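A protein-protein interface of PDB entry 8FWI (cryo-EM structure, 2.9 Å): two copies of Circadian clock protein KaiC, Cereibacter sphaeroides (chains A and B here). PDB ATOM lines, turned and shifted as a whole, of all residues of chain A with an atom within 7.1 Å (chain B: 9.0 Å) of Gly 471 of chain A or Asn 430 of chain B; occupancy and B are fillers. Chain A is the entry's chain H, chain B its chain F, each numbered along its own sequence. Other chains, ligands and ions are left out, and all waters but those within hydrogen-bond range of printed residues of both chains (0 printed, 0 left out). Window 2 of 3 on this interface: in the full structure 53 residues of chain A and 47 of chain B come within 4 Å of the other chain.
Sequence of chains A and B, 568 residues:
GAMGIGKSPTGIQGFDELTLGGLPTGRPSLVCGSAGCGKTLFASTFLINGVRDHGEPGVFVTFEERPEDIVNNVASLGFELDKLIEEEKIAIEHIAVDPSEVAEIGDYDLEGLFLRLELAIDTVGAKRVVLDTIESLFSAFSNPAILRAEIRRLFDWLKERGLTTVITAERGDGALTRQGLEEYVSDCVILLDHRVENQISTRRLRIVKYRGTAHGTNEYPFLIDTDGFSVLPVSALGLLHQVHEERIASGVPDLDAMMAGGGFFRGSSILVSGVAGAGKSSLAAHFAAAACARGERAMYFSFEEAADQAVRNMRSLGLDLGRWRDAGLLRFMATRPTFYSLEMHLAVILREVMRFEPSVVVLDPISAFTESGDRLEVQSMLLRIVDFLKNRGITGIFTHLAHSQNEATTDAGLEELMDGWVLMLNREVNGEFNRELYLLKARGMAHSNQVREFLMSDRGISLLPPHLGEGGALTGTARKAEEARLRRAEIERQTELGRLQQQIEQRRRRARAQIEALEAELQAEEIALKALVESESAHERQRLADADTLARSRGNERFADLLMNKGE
The side-chain amide oxygen (OD1) of Asn 430 of chain B sits close to the backbone carbonyl oxygen (O) of Gly 471 of chain A (3.0 Å).
The side-chain amide oxygen (OD1) of Asn 430 of chain B lies within hydrogen-bond range of the backbone NH (N) of Ala 473 of chain A, at 3.2 Å.
OE1 of Gln 450 of chain A lies close to O of Gly 431 of chain B (3.3 Å).
The backbone carbonyl oxygen (O) of Gly 431 of chain B is in hydrogen-bond range of the backbone NH (N) of Val 451 of chain A (3.1 Å).
The side-chain carboxylate (OE1) of Glu 432 of chain B is in hydrogen-bond range of the side-chain amide nitrogen (NE2) of Gln 450 of chain A, 3.4 Å away.
The side-chain carboxylate (OE2) of Glu 432 of chain B lies within hydrogen-bond range of the backbone NH (N) of Thr 477 of chain B (2.9 Å).
Glu 428 of chain B touches Val 451 of chain A (OE2 to CG2, 3.7 Å).
CG2 of Val 451 of chain A touches CE1 of Phe 433 of chain B (3.4 Å).
Gly 472 of chain A touches Asn 430 of chain B (C to OD1, 3.2 Å).
N of Gly 431 of chain B touches CB of Ala 473 of chain A, 3.8 Å away.
Printed residues of chain B within 4 Å of Val 451 of chain A: Glu 428 (3.7 Å), Gly 431 (3.1 Å) and Phe 433 (3.4 Å).
Gly 471 of chain A touches just one residue of chain B: Asn 430.
Of the printed residues of chain B, Gly 472 of chain A touches Asn 430.
Asn 430 of chain B touches three residues of chain A.
Of the printed residues of chain A, Glu 432 of chain B touches Gln 450 (3.4 Å).
The nearest printed residue of chain A that does not touch Phe 433 of chain B is Gln 450 of chain A (5.1 Å).
Of the 11 printed residues of chain A, 5 touch a printed residue of chain B.
Hydrophobic or aromatic side chains of chain A within 4 Å of the printed part of chain B: Val 451 and Ala 473.
Of the 18 printed residues of chain B, 5 touch a printed residue of chain A.
Printed residues of chain B that touch a printed residue of chain A: Glu 428, Asn 430, Gly 431, Glu 432 and Phe 433.
Hydrophobic or aromatic side chains of chain B that line the printed part of chain A: Phe 433.
Among the printed residues, no Asp or Glu carboxylate lies within 4 Å of a Lys or Arg side-chain nitrogen of the other chain.
2 positions are printed for both chains.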
ATOM      1  N   GLN A 450      -1.025 -18.376   3.428  1.00  0.00           N
ATOM      2  CA  GLN A 450      -0.150 -17.535   4.229  1.00  0.00           C
ATOM      3  C   GLN A 450       1.281 -18.051   4.174  1.00  0.00           C
ATOM      4  O   GLN A 450       1.519 -19.260   4.220  1.00  0.00           O
ATOM      5  CB  GLN A 450      -0.623 -17.492   5.682  1.00  0.00           C
ATOM      6  CG  GLN A 450      -2.041 -16.989   5.859  1.00  0.00           C
ATOM      7  CD  GLN A 450      -2.177 -15.518   5.535  1.00  0.00           C
ATOM      8  OE1 GLN A 450      -1.253 -14.735   5.747  1.00  0.00           O
ATOM      9  NE2 GLN A 450      -3.336 -15.133   5.017  1.00  0.00           N
ATOM     10  N   VAL A 451       2.230 -17.123   4.077  1.00  0.00           N
ATOM     11  CA  VAL A 451       3.654 -17.453   4.143  1.00  0.00           C
ATOM     12  C   VAL A 451       4.021 -17.408   5.623  1.00  0.00           C
ATOM     13  O   VAL A 451       4.365 -16.362   6.174  1.00  0.00           O
ATOM     14  CB  VAL A 451       4.505 -16.508   3.301  1.00  0.00           C
ATOM     15  CG1 VAL A 451       5.981 -16.766   3.544  1.00  0.00           C
ATOM     16  CG2 VAL A 451       4.167 -16.663   1.832  1.00  0.00           C
ATOM     17  N   HIS A 467       0.831 -13.361  11.633  1.00  0.00           N
ATOM     18  CA  HIS A 467       1.191 -11.970  11.858  1.00  0.00           C
ATOM     19  C   HIS A 467      -0.020 -11.084  11.617  1.00  0.00           C
ATOM     20  O   HIS A 467      -0.596 -11.098  10.522  1.00  0.00           O
ATOM     21  CB  HIS A 467       2.323 -11.545  10.936  1.00  0.00           C
ATOM     22  CG  HIS A 467       2.917 -10.223  11.296  1.00  0.00           C
ATOM     23  ND1 HIS A 467       2.320  -9.026  10.969  1.00  0.00           N
ATOM     24  CD2 HIS A 467       4.039  -9.908  11.979  1.00  0.00           C
ATOM     25  CE1 HIS A 467       3.057  -8.029  11.426  1.00  0.00           C
ATOM     26  NE2 HIS A 467       4.107  -8.537  12.043  1.00  0.00           N
ATOM     27  N   LEU A 468      -0.396 -10.300  12.626  1.00  0.00           N
ATOM     28  CA  LEU A 468      -1.537  -9.399  12.509  1.00  0.00           C
ATOM     29  C   LEU A 468      -1.064  -7.977  12.729  1.00  0.00           C
ATOM     30  O   LEU A 468      -0.661  -7.610  13.839  1.00  0.00           O
ATOM     31  CB  LEU A 468      -2.624  -9.764  13.500  1.00  0.00           C
ATOM     32  CG  LEU A 468      -3.114 -11.094  12.951  1.00  0.00           C
ATOM     33  CD1 LEU A 468      -2.844 -12.225  13.917  1.00  0.00           C
ATOM     34  CD2 LEU A 468      -4.523 -11.168  12.573  1.00  0.00           C
ATOM     35  N   GLY A 469      -1.117  -7.187  11.669  1.00  0.00           N
ATOM     36  CA  GLY A 469      -0.801  -5.780  11.753  1.00  0.00           C
ATOM     37  C   GLY A 469      -1.146  -5.150  10.429  1.00  0.00           C
ATOM     38  O   GLY A 469      -1.241  -5.832   9.404  1.00  0.00           O
ATOM     39  N   GLU A 470      -1.339  -3.836  10.457  1.00  0.00           N
ATOM     40  CA  GLU A 470      -1.774  -3.173   9.238  1.00  0.00           C
ATOM     41  C   GLU A 470      -0.700  -3.283   8.167  1.00  0.00           C
ATOM     42  O   GLU A 470      -0.999  -3.480   6.983  1.00  0.00           O
ATOM     43  CB  GLU A 470      -2.138  -1.721   9.515  1.00  0.00           C
ATOM     44  CG  GLU A 470      -3.363  -1.668  10.418  1.00  0.00           C
ATOM     45  CD  GLU A 470      -3.019  -1.794  11.897  1.00  0.00           C
ATOM     46  OE1 GLU A 470      -1.814  -1.859  12.223  1.00  0.00           O
ATOM     47  OE2 GLU A 470      -3.949  -1.820  12.731  1.00  0.00           O
ATOM     48  N   GLY A 471       0.563  -3.158   8.570  1.00  0.00           N
ATOM     49  CA  GLY A 471       1.650  -3.379   7.633  1.00  0.00           C
ATOM     50  C   GLY A 471       1.831  -4.846   7.286  1.00  0.00           C
ATOM     51  O   GLY A 471       1.907  -5.216   6.111  1.00  0.00           O
ATOM     52  N   GLY A 472       1.901  -5.702   8.304  1.00  0.00           N
ATOM     53  CA  GLY A 472       2.099  -7.122   8.088  1.00  0.00           C
ATOM     54  C   GLY A 472       3.457  -7.453   7.502  1.00  0.00           C
ATOM     55  O   GLY A 472       4.297  -6.567   7.316  1.00  0.00           O
ATOM     56  N   ALA A 473       3.680  -8.733   7.202  1.00  0.00           N
ATOM     57  CA  ALA A 473       4.875  -9.182   6.486  1.00  0.00           C
ATOM     58  C   ALA A 473       6.160  -8.800   7.213  1.00  0.00           C
ATOM     59  O   ALA A 473       7.145  -8.387   6.595  1.00  0.00           O
ATOM     60  CB  ALA A 473       4.891  -8.632   5.061  1.00  0.00           C
ATOM     61  N   LEU A 474       6.158  -8.935   8.533  1.00  0.00           N
ATOM     62  CA  LEU A 474       7.360  -8.766   9.335  1.00  0.00           C
ATOM     63  C   LEU A 474       7.660 -10.066  10.063  1.00  0.00           C
ATOM     64  O   LEU A 474       6.748 -10.739  10.554  1.00  0.00           O
ATOM     65  CB  LEU A 474       7.204  -7.618  10.327  1.00  0.00           C
ATOM     66  CG  LEU A 474       7.173  -6.236   9.677  1.00  0.00           C
ATOM     67  CD1 LEU A 474       6.729  -5.231  10.685  1.00  0.00           C
ATOM     68  CD2 LEU A 474       8.535  -5.843   9.134  1.00  0.00           C
ATOM     69  N   GLU A 482       8.047  -4.042  16.105  1.00  0.00           N
ATOM     70  CA  GLU A 482       6.781  -3.404  15.770  1.00  0.00           C
ATOM     71  C   GLU A 482       5.752  -3.592  16.874  1.00  0.00           C
ATOM     72  O   GLU A 482       4.941  -2.695  17.128  1.00  0.00           O
ATOM     73  CB  GLU A 482       6.251  -3.941  14.445  1.00  0.00           C
ATOM     74  CG  GLU A 482       6.782  -3.190  13.244  1.00  0.00           C
ATOM     75  CD  GLU A 482       6.383  -1.726  13.237  1.00  0.00           C
ATOM     76  OE1 GLU A 482       5.211  -1.427  13.542  1.00  0.00           O
ATOM     77  OE2 GLU A 482       7.244  -0.876  12.928  1.00  0.00           O
ATOM     78  N   ARG B 427       0.439 -14.366  -6.701  1.00  0.00           N
ATOM     79  CA  ARG B 427       1.639 -13.641  -6.316  1.00  0.00           C
ATOM     80  C   ARG B 427       1.683 -13.423  -4.811  1.00  0.00           C
ATOM     81  O   ARG B 427       0.667 -13.498  -4.119  1.00  0.00           O
ATOM     82  CB  ARG B 427       1.706 -12.288  -7.027  1.00  0.00           C
ATOM     83  CG  ARG B 427       1.697 -12.391  -8.535  1.00  0.00           C
ATOM     84  CD  ARG B 427       1.965 -11.050  -9.182  1.00  0.00           C
ATOM     85  NE  ARG B 427       0.816 -10.156  -9.101  1.00  0.00           N
ATOM     86  CZ  ARG B 427       0.487  -9.262 -10.026  1.00  0.00           C
ATOM     87  NH1 ARG B 427       1.201  -9.113 -11.130  1.00  0.00           N
ATOM     88  NH2 ARG B 427      -0.583  -8.497  -9.836  1.00  0.00           N
ATOM     89  N   GLU B 428       2.883 -13.121  -4.314  1.00  0.00           N
ATOM     90  CA  GLU B 428       3.127 -12.895  -2.893  1.00  0.00           C
ATOM     91  C   GLU B 428       3.186 -11.399  -2.626  1.00  0.00           C
ATOM     92  O   GLU B 428       4.041 -10.696  -3.174  1.00  0.00           O
ATOM     93  CB  GLU B 428       4.423 -13.552  -2.434  1.00  0.00           C
ATOM     94  CG  GLU B 428       4.622 -13.497  -0.928  1.00  0.00           C
ATOM     95  CD  GLU B 428       5.963 -14.054  -0.494  1.00  0.00           C
ATOM     96  OE1 GLU B 428       6.661 -14.651  -1.338  1.00  0.00           O
ATOM     97  OE2 GLU B 428       6.316 -13.894   0.694  1.00  0.00           O
ATOM     98  N   VAL B 429       2.274 -10.921  -1.787  1.00  0.00           N
ATOM     99  CA  VAL B 429       2.340  -9.574  -1.241  1.00  0.00           C
ATOM    100  C   VAL B 429       1.888  -9.647   0.210  1.00  0.00           C
ATOM    101  O   VAL B 429       0.838 -10.219   0.515  1.00  0.00           O
ATOM    102  CB  VAL B 429       1.467  -8.590  -2.048  1.00  0.00           C
ATOM    103  CG1 VAL B 429       1.403  -7.235  -1.359  1.00  0.00           C
ATOM    104  CG2 VAL B 429       2.000  -8.450  -3.467  1.00  0.00           C
ATOM    105  N   ASN B 430       2.685  -9.067   1.104  1.00  0.00           N
ATOM    106  CA  ASN B 430       2.312  -8.949   2.513  1.00  0.00           C
ATOM    107  C   ASN B 430       2.205 -10.320   3.185  1.00  0.00           C
ATOM    108  O   ASN B 430       1.291 -10.581   3.971  1.00  0.00           O
ATOM    109  CB  ASN B 430       1.001  -8.174   2.649  1.00  0.00           C
ATOM    110  CG  ASN B 430       0.694  -7.774   4.070  1.00  0.00           C
ATOM    111  OD1 ASN B 430       1.509  -7.960   4.972  1.00  0.00           O
ATOM    112  ND2 ASN B 430      -0.498  -7.226   4.279  1.00  0.00           N
ATOM    113  N   GLY B 431       3.149 -11.205   2.882  1.00  0.00           N
ATOM    114  CA  GLY B 431       3.176 -12.505   3.532  1.00  0.00           C
ATOM    115  C   GLY B 431       1.966 -13.363   3.247  1.00  0.00           C
ATOM    116  O   GLY B 431       1.533 -14.127   4.115  1.00  0.00           O
ATOM    117  N   GLU B 432       1.407 -13.259   2.046  1.00  0.00           N
ATOM    118  CA  GLU B 432       0.290 -14.092   1.632  1.00  0.00           C
ATOM    119  C   GLU B 432       0.285 -14.129   0.115  1.00  0.00           C
ATOM    120  O   GLU B 432       0.818 -13.233  -0.545  1.00  0.00           O
ATOM    121  CB  GLU B 432      -1.046 -13.563   2.161  1.00  0.00           C
ATOM    122  CG  GLU B 432      -1.347 -12.138   1.742  1.00  0.00           C
ATOM    123  CD  GLU B 432      -2.566 -11.559   2.433  1.00  0.00           C
ATOM    124  OE1 GLU B 432      -2.985 -12.108   3.474  1.00  0.00           O
ATOM    125  OE2 GLU B 432      -3.093 -10.537   1.946  1.00  0.00           O
ATOM    126  N   PHE B 433      -0.328 -15.171  -0.433  1.00  0.00           N
ATOM    127  CA  PHE B 433      -0.435 -15.342  -1.873  1.00  0.00           C
ATOM    128  C   PHE B 433      -1.876 -15.103  -2.294  1.00  0.00           C
ATOM    129  O   PHE B 433      -2.791 -15.772  -1.799  1.00  0.00           O
ATOM    130  CB  PHE B 433       0.034 -16.735  -2.297  1.00  0.00           C
ATOM    131  CG  PHE B 433       1.522 -16.850  -2.467  1.00  0.00           C
ATOM    132  CD1 PHE B 433       2.345 -17.026  -1.371  1.00  0.00           C
ATOM    133  CD2 PHE B 433       2.098 -16.777  -3.725  1.00  0.00           C
ATOM    134  CE1 PHE B 433       3.712 -17.132  -1.522  1.00  0.00           C
ATOM    135  CE2 PHE B 433       3.467 -16.882  -3.881  1.00  0.00           C
ATOM    136  CZ  PHE B 433       4.273 -17.063  -2.778  1.00  0.00           C
ATOM    137  N   ASN B 434      -2.076 -14.148  -3.202  1.00  0.00           N
ATOM    138  CA  ASN B 434      -3.399 -13.752  -3.660  1.00  0.00           C
ATOM    139  C   ASN B 434      -3.562 -14.086  -5.134  1.00  0.00           C
ATOM    140  O   ASN B 434      -2.642 -13.883  -5.933  1.00  0.00           O
ATOM    141  CB  ASN B 434      -3.632 -12.254  -3.446  1.00  0.00           C
ATOM    142  CG  ASN B 434      -3.622 -11.867  -1.984  1.00  0.00           C
ATOM    143  OD1 ASN B 434      -4.390 -12.393  -1.184  1.00  0.00           O
ATOM    144  ND2 ASN B 434      -2.749 -10.931  -1.629  1.00  0.00           N
ATOM    145  N   LEU B 474      -4.539  -2.824  -4.185  1.00  0.00           N
ATOM    146  CA  LEU B 474      -4.354  -3.575  -2.954  1.00  0.00           C
ATOM    147  C   LEU B 474      -5.252  -4.802  -2.980  1.00  0.00           C
ATOM    148  O   LEU B 474      -6.400  -4.734  -3.431  1.00  0.00           O
ATOM    149  CB  LEU B 474      -4.659  -2.714  -1.733  1.00  0.00           C
ATOM    150  CG  LEU B 474      -3.630  -1.613  -1.479  1.00  0.00           C
ATOM    151  CD1 LEU B 474      -4.168  -0.667  -0.460  1.00  0.00           C
ATOM    152  CD2 LEU B 474      -2.310  -2.182  -0.994  1.00  0.00           C
ATOM    153  N   THR B 475      -4.721  -5.922  -2.498  1.00  0.00           N
ATOM    154  CA  THR B 475      -5.398  -7.207  -2.576  1.00  0.00           C
ATOM    155  C   THR B 475      -5.364  -7.897  -1.224  1.00  0.00           C
ATOM    156  O   THR B 475      -4.462  -7.672  -0.412  1.00  0.00           O
ATOM    157  CB  THR B 475      -4.746  -8.121  -3.619  1.00  0.00           C
ATOM    158  OG1 THR B 475      -3.386  -8.377  -3.249  1.00  0.00           O
ATOM    159  CG2 THR B 475      -4.776  -7.481  -4.992  1.00  0.00           C
ATOM    160  N   GLY B 476      -6.363  -8.743  -0.990  1.00  0.00           N
ATOM    161  CA  GLY B 476      -6.372  -9.596   0.179  1.00  0.00           C
ATOM    162  C   GLY B 476      -6.522  -8.848   1.485  1.00  0.00           C
ATOM    163  O   GLY B 476      -7.478  -8.091   1.677  1.00  0.00           O
ATOM    164  N   THR B 477      -5.576  -9.064   2.400  1.00  0.00           N
ATOM    165  CA  THR B 477      -5.669  -8.469   3.727  1.00  0.00           C
ATOM    166  C   THR B 477      -5.387  -6.972   3.695  1.00  0.00           C
ATOM    167  O   THR B 477      -6.013  -6.205   4.434  1.00  0.00           O
ATOM    168  CB  THR B 477      -4.700  -9.171   4.680  1.00  0.00           C
ATOM    169  OG1 THR B 477      -5.181 -10.489   4.968  1.00  0.00           O
ATOM    170  CG2 THR B 477      -4.566  -8.393   5.974  1.00  0.00           C
ATOM    171  N   ALA B 478      -4.451  -6.536   2.849  1.00  0.00           N
ATOM    172  CA  ALA B 478      -4.141  -5.113   2.766  1.00  0.00           C
ATOM    173  C   ALA B 478      -5.367  -4.299   2.384  1.00  0.00           C
ATOM    174  O   ALA B 478      -5.509  -3.148   2.816  1.00  0.00           O
ATOM    175  CB  ALA B 478      -3.016  -4.879   1.762  1.00  0.00           C
ATOM    176  N   ARG B 479      -6.259  -4.872   1.576  1.00  0.00           N
ATOM    177  CA  ARG B 479      -7.486  -4.177   1.210  1.00  0.00           C
ATOM    178  C   ARG B 479      -8.334  -3.886   2.442  1.00  0.00           C
ATOM    179  O   ARG B 479      -8.807  -2.758   2.638  1.00  0.00           O
ATOM    180  CB  ARG B 479      -8.264  -5.019   0.199  1.00  0.00           C
ATOM    181  CG  ARG B 479      -9.440  -4.321  -0.448  1.00  0.00           C
ATOM    182  CD  ARG B 479     -10.414  -5.328  -1.035  1.00  0.00           C
ATOM    183  NE  ARG B 479     -11.430  -4.692  -1.869  1.00  0.00           N
ATOM    184  CZ  ARG B 479     -11.667  -4.985  -3.142  1.00  0.00           C
ATOM    185  NH1 ARG B 479     -10.972  -5.907  -3.789  1.00  0.00           N
ATOM    186  NH2 ARG B 479     -12.629  -4.331  -3.788  1.00  0.00           N
ATOM    187  N   LYS B 480      -8.521  -4.893   3.297  1.00  0.00           N
ATOM    188  CA  LYS B 480      -9.315  -4.688   4.502  1.00  0.00           C
ATOM    189  C   LYS B 480      -8.640  -3.690   5.434  1.00  0.00           C
ATOM    190  O   LYS B 480      -9.308  -2.856   6.061  1.00  0.00           O
ATOM    191  CB  LYS B 480      -9.538  -6.016   5.218  1.00  0.00           C
ATOM    192  CG  LYS B 480     -10.341  -7.027   4.430  1.00  0.00           C
ATOM    193  CD  LYS B 480     -10.583  -8.284   5.266  1.00  0.00           C
ATOM    194  CE  LYS B 480     -11.467  -9.312   4.580  1.00  0.00           C
ATOM    195  NZ  LYS B 480     -11.220  -9.700   3.159  1.00  0.00           N
ATOM    196  N   ALA B 481      -7.312  -3.763   5.540  1.00  0.00           N
ATOM    197  CA  ALA B 481      -6.583  -2.822   6.379  1.00  0.00           C
ATOM    198  C   ALA B 481      -6.804  -1.389   5.912  1.00  0.00           C
ATOM    199  O   ALA B 481      -7.030  -0.486   6.728  1.00  0.00           O
ATOM    200  CB  ALA B 481      -5.094  -3.166   6.371  1.00  0.00           C
ATOM    201  N   GLU B 482      -6.753  -1.162   4.600  1.00  0.00           N
ATOM    202  CA  GLU B 482      -6.961   0.187   4.086  1.00  0.00           C
ATOM    203  C   GLU B 482      -8.405   0.635   4.263  1.00  0.00           C
ATOM    204  O   GLU B 482      -8.661   1.815   4.519  1.00  0.00           O
ATOM    205  CB  GLU B 482      -6.552   0.264   2.620  1.00  0.00           C
ATOM    206  CG  GLU B 482      -5.082   0.575   2.429  1.00  0.00           C
ATOM    207  CD  GLU B 482      -4.682   1.921   2.998  1.00  0.00           C
ATOM    208  OE1 GLU B 482      -5.436   2.898   2.801  1.00  0.00           O
ATOM    209  OE2 GLU B 482      -3.616   2.002   3.643  1.00  0.00           O
ATOM    210  N   ARG B 488     -11.364   5.003   9.860  1.00  0.00           N
ATOM    211  CA  ARG B 488     -10.813   5.721  11.004  1.00  0.00           C
ATOM    212  C   ARG B 488     -10.587   7.193  10.675  1.00  0.00           C
ATOM    213  O   ARG B 488     -10.898   8.077  11.484  1.00  0.00           O
ATOM    214  CB  ARG B 488      -9.507   5.065  11.448  1.00  0.00           C
ATOM    215  CG  ARG B 488      -9.690   3.918  12.431  1.00  0.00           C
ATOM    216  CD  ARG B 488      -8.417   3.652  13.219  1.00  0.00           C
ATOM    217  NE  ARG B 488      -7.265   3.450  12.349  1.00  0.00           N
ATOM    218  CZ  ARG B 488      -6.808   2.266  11.960  1.00  0.00           C
ATOM    219  NH1 ARG B 488      -7.384   1.139  12.342  1.00  0.00           N
ATOM    220  NH2 ARG B 488      -5.744   2.213  11.165  1.00  0.00           N
